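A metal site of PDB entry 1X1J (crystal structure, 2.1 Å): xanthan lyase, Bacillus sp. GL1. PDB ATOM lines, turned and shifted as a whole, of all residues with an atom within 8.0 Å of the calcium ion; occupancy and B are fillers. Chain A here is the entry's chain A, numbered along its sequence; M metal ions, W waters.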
ATOM      1  N   TYR A 466      10.860 -22.849 -21.257  1.00  0.00           N
ATOM      2  CA  TYR A 466      10.780 -21.645 -20.444  1.00  0.00           C
ATOM      3  C   TYR A 466       9.520 -20.909 -20.860  1.00  0.00           C
ATOM      4  O   TYR A 466       8.848 -21.323 -21.806  1.00  0.00           O
ATOM      5  CB  TYR A 466      11.994 -20.729 -20.708  1.00  0.00           C
ATOM      6  CG  TYR A 466      13.311 -21.445 -20.638  1.00  0.00           C
ATOM      7  CD1 TYR A 466      13.975 -21.852 -21.799  1.00  0.00           C
ATOM      8  CD2 TYR A 466      13.901 -21.755 -19.409  1.00  0.00           C
ATOM      9  CE1 TYR A 466      15.170 -22.551 -21.747  1.00  0.00           C
ATOM     10  CE2 TYR A 466      15.096 -22.459 -19.335  1.00  0.00           C
ATOM     11  CZ  TYR A 466      15.733 -22.846 -20.516  1.00  0.00           C
ATOM     12  OH  TYR A 466      16.917 -23.542 -20.458  1.00  0.00           O
ATOM     13  N   PHE A 489      12.215 -19.169 -15.635  1.00  0.00           N
ATOM     14  CA  PHE A 489      13.467 -19.625 -16.190  1.00  0.00           C
ATOM     15  C   PHE A 489      13.819 -20.997 -15.629  1.00  0.00           C
ATOM     16  O   PHE A 489      12.912 -21.772 -15.312  1.00  0.00           O
ATOM     17  CB  PHE A 489      14.542 -18.575 -15.905  1.00  0.00           C
ATOM     18  CG  PHE A 489      14.257 -17.248 -16.560  1.00  0.00           C
ATOM     19  CD1 PHE A 489      14.371 -16.055 -15.849  1.00  0.00           C
ATOM     20  CD2 PHE A 489      13.839 -17.190 -17.890  1.00  0.00           C
ATOM     21  CE1 PHE A 489      14.080 -14.819 -16.444  1.00  0.00           C
ATOM     22  CE2 PHE A 489      13.553 -15.963 -18.504  1.00  0.00           C
ATOM     23  CZ  PHE A 489      13.669 -14.782 -17.778  1.00  0.00           C
ATOM     24  N   ASP A 490      15.109 -21.310 -15.521  1.00  0.00           N
ATOM     25  CA  ASP A 490      15.500 -22.626 -15.026  1.00  0.00           C
ATOM     26  C   ASP A 490      15.379 -22.860 -13.525  1.00  0.00           C
ATOM     27  O   ASP A 490      14.694 -23.784 -13.091  1.00  0.00           O
ATOM     28  CB  ASP A 490      16.919 -22.975 -15.492  1.00  0.00           C
ATOM     29  CG  ASP A 490      17.956 -21.936 -15.097  1.00  0.00           C
ATOM     30  OD1 ASP A 490      19.159 -22.249 -15.200  1.00  0.00           O
ATOM     31  OD2 ASP A 490      17.578 -20.809 -14.680  1.00  0.00           O
ATOM     32  N   ASP A 491      16.033 -22.017 -12.735  1.00  0.00           N
ATOM     33  CA  ASP A 491      16.024 -22.161 -11.286  1.00  0.00           C
ATOM     34  C   ASP A 491      15.414 -20.972 -10.548  1.00  0.00           C
ATOM     35  O   ASP A 491      15.470 -20.910  -9.321  1.00  0.00           O
ATOM     36  CB  ASP A 491      17.450 -22.422 -10.785  1.00  0.00           C
ATOM     37  CG  ASP A 491      18.388 -21.234 -11.029  1.00  0.00           C
ATOM     38  OD1 ASP A 491      18.205 -20.530 -12.047  1.00  0.00           O
ATOM     39  OD2 ASP A 491      19.305 -20.999 -10.218  1.00  0.00           O
ATOM     40  N   GLU A 492      14.843 -20.025 -11.284  1.00  0.00           N
ATOM     41  CA  GLU A 492      14.229 -18.854 -10.659  1.00  0.00           C
ATOM     42  C   GLU A 492      13.025 -18.335 -11.431  1.00  0.00           C
ATOM     43  O   GLU A 492      12.879 -18.574 -12.636  1.00  0.00           O
ATOM     44  CB  GLU A 492      15.253 -17.714 -10.513  1.00  0.00           C
ATOM     45  CG  GLU A 492      15.530 -16.919 -11.789  1.00  0.00           C
ATOM     46  CD  GLU A 492      16.689 -17.467 -12.598  1.00  0.00           C
ATOM     47  OE1 GLU A 492      17.829 -16.966 -12.453  1.00  0.00           O
ATOM     48  OE2 GLU A 492      16.465 -18.415 -13.385  1.00  0.00           O
ATOM     49  N   ILE A 493      12.152 -17.632 -10.732  1.00  0.00           N
ATOM     50  CA  ILE A 493      10.981 -17.039 -11.343  1.00  0.00           C
ATOM     51  C   ILE A 493      10.996 -15.572 -10.940  1.00  0.00           C
ATOM     52  O   ILE A 493      11.049 -15.246  -9.757  1.00  0.00           O
ATOM     53  CB  ILE A 493       9.660 -17.683 -10.835  1.00  0.00           C
ATOM     54  CG1 ILE A 493       9.668 -19.190 -11.108  1.00  0.00           C
ATOM     55  CG2 ILE A 493       8.474 -17.050 -11.553  1.00  0.00           C
ATOM     56  CD1 ILE A 493       9.963 -20.028  -9.882  1.00  0.00           C
ATOM     57  N   VAL A 618      12.533 -11.984  -7.170  1.00  0.00           N
ATOM     58  CA  VAL A 618      12.865 -13.257  -7.800  1.00  0.00           C
ATOM     59  C   VAL A 618      12.735 -14.399  -6.803  1.00  0.00           C
ATOM     60  O   VAL A 618      13.308 -14.350  -5.709  1.00  0.00           O
ATOM     61  CB  VAL A 618      14.325 -13.249  -8.335  1.00  0.00           C
ATOM     62  CG1 VAL A 618      14.585 -14.473  -9.180  1.00  0.00           C
ATOM     63  CG2 VAL A 618      14.581 -11.973  -9.128  1.00  0.00           C
ATOM     64  N   LEU A 620      13.698 -17.965  -5.618  1.00  0.00           N
ATOM     65  CA  LEU A 620      14.805 -18.901  -5.788  1.00  0.00           C
ATOM     66  C   LEU A 620      14.497 -20.174  -5.009  1.00  0.00           C
ATOM     67  O   LEU A 620      14.903 -20.331  -3.863  1.00  0.00           O
ATOM     68  CB  LEU A 620      16.097 -18.262  -5.266  1.00  0.00           C
ATOM     69  CG  LEU A 620      16.487 -16.899  -5.880  1.00  0.00           C
ATOM     70  CD1 LEU A 620      17.685 -16.325  -5.140  1.00  0.00           C
ATOM     71  CD2 LEU A 620      16.790 -17.044  -7.352  1.00  0.00           C
ATOM     72  N   LYS A 623      17.222 -23.065  -2.663  1.00  0.00           N
ATOM     73  CA  LYS A 623      18.621 -22.634  -2.513  1.00  0.00           C
ATOM     74  C   LYS A 623      18.909 -22.394  -1.017  1.00  0.00           C
ATOM     75  O   LYS A 623      18.019 -21.955  -0.284  1.00  0.00           O
ATOM     76  CB  LYS A 623      18.869 -21.342  -3.281  1.00  0.00           C
ATOM     77  CG  LYS A 623      19.358 -21.545  -4.701  1.00  0.00           C
ATOM     78  CD  LYS A 623      19.488 -20.203  -5.425  1.00  0.00           C
ATOM     79  CE  LYS A 623      20.229 -20.360  -6.753  1.00  0.00           C
ATOM     80  NZ  LYS A 623      19.667 -21.502  -7.527  1.00  0.00           N
ATOM     81  N   TYR A 631      23.758 -15.691  -5.258  1.00  0.00           N
ATOM     82  CA  TYR A 631      22.943 -15.252  -6.380  1.00  0.00           C
ATOM     83  C   TYR A 631      22.824 -13.743  -6.300  1.00  0.00           C
ATOM     84  O   TYR A 631      23.037 -13.029  -7.275  1.00  0.00           O
ATOM     85  CB  TYR A 631      21.545 -15.866  -6.301  1.00  0.00           C
ATOM     86  CG  TYR A 631      20.692 -15.598  -7.517  1.00  0.00           C
ATOM     87  CD1 TYR A 631      20.693 -16.472  -8.613  1.00  0.00           C
ATOM     88  CD2 TYR A 631      19.877 -14.459  -7.596  1.00  0.00           C
ATOM     89  CE1 TYR A 631      19.916 -16.232  -9.737  1.00  0.00           C
ATOM     90  CE2 TYR A 631      19.095 -14.206  -8.722  1.00  0.00           C
ATOM     91  CZ  TYR A 631      19.129 -15.087  -9.791  1.00  0.00           C
ATOM     92  OH  TYR A 631      18.368 -14.834 -10.907  1.00  0.00           O
ATOM     93  N   PRO A 635      23.511 -11.914  -9.701  1.00  0.00           N
ATOM     94  CA  PRO A 635      22.256 -12.479 -10.212  1.00  0.00           C
ATOM     95  C   PRO A 635      22.279 -12.854 -11.696  1.00  0.00           C
ATOM     96  O   PRO A 635      22.844 -12.151 -12.523  1.00  0.00           O
ATOM     97  CB  PRO A 635      21.232 -11.399  -9.874  1.00  0.00           C
ATOM     98  CG  PRO A 635      22.018 -10.145  -9.994  1.00  0.00           C
ATOM     99  CD  PRO A 635      23.322 -10.500  -9.305  1.00  0.00           C
ATOM    100  N   ALA A 636      21.638 -13.982 -12.008  1.00  0.00           N
ATOM    101  CA  ALA A 636      21.570 -14.462 -13.378  1.00  0.00           C
ATOM    102  C   ALA A 636      20.552 -13.695 -14.225  1.00  0.00           C
ATOM    103  O   ALA A 636      20.665 -13.663 -15.447  1.00  0.00           O
ATOM    104  CB  ALA A 636      21.219 -15.952 -13.391  1.00  0.00           C
ATOM    105  N   ILE A 637      19.564 -13.071 -13.589  1.00  0.00           N
ATOM    106  CA  ILE A 637      18.556 -12.305 -14.313  1.00  0.00           C
ATOM    107  C   ILE A 637      18.792 -10.806 -14.236  1.00  0.00           C
ATOM    108  O   ILE A 637      19.439 -10.314 -13.316  1.00  0.00           O
ATOM    109  CB  ILE A 637      17.102 -12.601 -13.803  1.00  0.00           C
ATOM    110  CG1 ILE A 637      16.944 -12.132 -12.354  1.00  0.00           C
ATOM    111  CG2 ILE A 637      16.790 -14.076 -13.949  1.00  0.00           C
ATOM    112  CD1 ILE A 637      16.440 -10.696 -12.202  1.00  0.00           C
ATOM    113  N   GLU A 651      17.721 -13.311 -18.852  1.00  0.00           N
ATOM    114  CA  GLU A 651      18.392 -14.321 -18.053  1.00  0.00           C
ATOM    115  C   GLU A 651      19.734 -14.482 -18.743  1.00  0.00           C
ATOM    116  O   GLU A 651      19.864 -15.205 -19.723  1.00  0.00           O
ATOM    117  CB  GLU A 651      17.608 -15.639 -18.055  1.00  0.00           C
ATOM    118  CG  GLU A 651      17.759 -16.471 -16.776  1.00  0.00           C
ATOM    119  CD  GLU A 651      19.164 -17.023 -16.562  1.00  0.00           C
ATOM    120  OE1 GLU A 651      19.388 -17.721 -15.547  1.00  0.00           O
ATOM    121  OE2 GLU A 651      20.060 -16.776 -17.405  1.00  0.00           O
ATOM    122  N   LYS A 652      20.718 -13.751 -18.228  1.00  0.00           N
ATOM    123  CA  LYS A 652      22.082 -13.713 -18.750  1.00  0.00           C
ATOM    124  C   LYS A 652      22.754 -15.046 -19.042  1.00  0.00           C
ATOM    125  O   LYS A 652      23.365 -15.206 -20.099  1.00  0.00           O
ATOM    126  CB  LYS A 652      22.945 -12.913 -17.763  1.00  0.00           C
ATOM    127  CG  LYS A 652      24.387 -12.729 -18.191  1.00  0.00           C
ATOM    128  CD  LYS A 652      25.190 -12.064 -17.068  1.00  0.00           C
ATOM    129  CE  LYS A 652      24.508 -10.786 -16.578  1.00  0.00           C
ATOM    130  NZ  LYS A 652      25.279 -10.120 -15.475  1.00  0.00           N
ATOM    131  N   THR A 653      22.682 -16.000 -18.116  1.00  0.00           N
ATOM    132  CA  THR A 653      23.322 -17.298 -18.301  1.00  0.00           C
ATOM    133  C   THR A 653      22.697 -18.176 -19.384  1.00  0.00           C
ATOM    134  O   THR A 653      23.349 -19.045 -19.944  1.00  0.00           O
ATOM    135  CB  THR A 653      23.314 -18.141 -16.991  1.00  0.00           C
ATOM    136  OG1 THR A 653      21.981 -18.598 -16.720  1.00  0.00           O
ATOM    137  CG2 THR A 653      23.808 -17.308 -15.819  1.00  0.00           C
ATOM    138  N   LEU A 654      21.419 -17.940 -19.676  1.00  0.00           N
ATOM    139  CA  LEU A 654      20.721 -18.754 -20.676  1.00  0.00           C
ATOM    140  C   LEU A 654      20.459 -18.018 -21.995  1.00  0.00           C
ATOM    141  O   LEU A 654      19.944 -18.606 -22.945  1.00  0.00           O
ATOM    142  CB  LEU A 654      19.395 -19.247 -20.106  1.00  0.00           C
ATOM    143  CG  LEU A 654      19.488 -20.017 -18.785  1.00  0.00           C
ATOM    144  CD1 LEU A 654      18.087 -20.290 -18.242  1.00  0.00           C
ATOM    145  CD2 LEU A 654      20.239 -21.321 -19.005  1.00  0.00           C
ATOM    146  N   LEU A 656      18.342 -15.774 -22.499  1.00  0.00           N
ATOM    147  CA  LEU A 656      16.901 -15.599 -22.634  1.00  0.00           C
ATOM    148  C   LEU A 656      16.443 -14.174 -22.360  1.00  0.00           C
ATOM    149  O   LEU A 656      16.920 -13.533 -21.428  1.00  0.00           O
ATOM    150  CB  LEU A 656      16.158 -16.529 -21.668  1.00  0.00           C
ATOM    151  CG  LEU A 656      16.223 -18.032 -21.884  1.00  0.00           C
ATOM    152  CD1 LEU A 656      15.704 -18.738 -20.628  1.00  0.00           C
ATOM    153  CD2 LEU A 656      15.382 -18.407 -23.101  1.00  0.00           C
HETATM  154 CA    CA M   1      18.949 -19.003 -13.550  1.00  0.00          CA
HETATM  155  O   HOH W   1      21.020 -20.425 -14.726  1.00  0.00           O
HETATM  156  O   HOH W   2      20.682 -18.850 -11.943  1.00  0.00           O
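The side-chain carboxylate (OD2) of Asp 491 lies within salt-bridge range of the side-chain amino group (NZ) of Lys 623 (2.8 Å).
The side-chain carboxylate (OE2) of Glu 651 is in hydrogen-bond range of the side-chain hydroxyl (OG1) of Thr 653 (2.7 Å).
The side-chain carboxylate (OE2) of Glu 651 is in hydrogen-bond range of the backbone NH (N) of Leu 654 (2.9 Å).
N of Glu 651 sits at hydrogen-bond distance from O of Leu 656, 2.7 Å away.
The side-chain hydroxyl (OH) of Tyr 631 sits close to the side-chain carboxylate (OE1) of Glu 492, 2.7 Å away.
The backbone carbonyl oxygen (O) of Ala 636 sits at hydrogen-bond distance from the backbone NH (N) of Lys 652 (2.8 Å).
The calcium ion is bound by the side-chain carboxylate (OD1) of Asp 491 (2.3 Å), water W2 (2.4 Å), the side-chain carboxylate (OE1) of Glu 651 (2.4 Å), the side-chain carboxylate (OD2) of Asp 490 (2.5 Å), the side-chain carboxylate (OE2) of Glu 492 (2.6 Å), the side-chain carboxylate (OE1) of Glu 492 (2.6 Å) and water W1 (2.8 Å).
Ala 636 touches the calcium ion.
Within 4 Å of the calcium ion: Asp 490, Asp 491, Glu 492, Ala 636 and Glu 651.
Water W1 lies within hydrogen-bond range of the side-chain carboxylate (OD1) of Asp 490 (2.6 Å) and the side-chain hydroxyl (OG1) of Thr 653 (2.9 Å).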
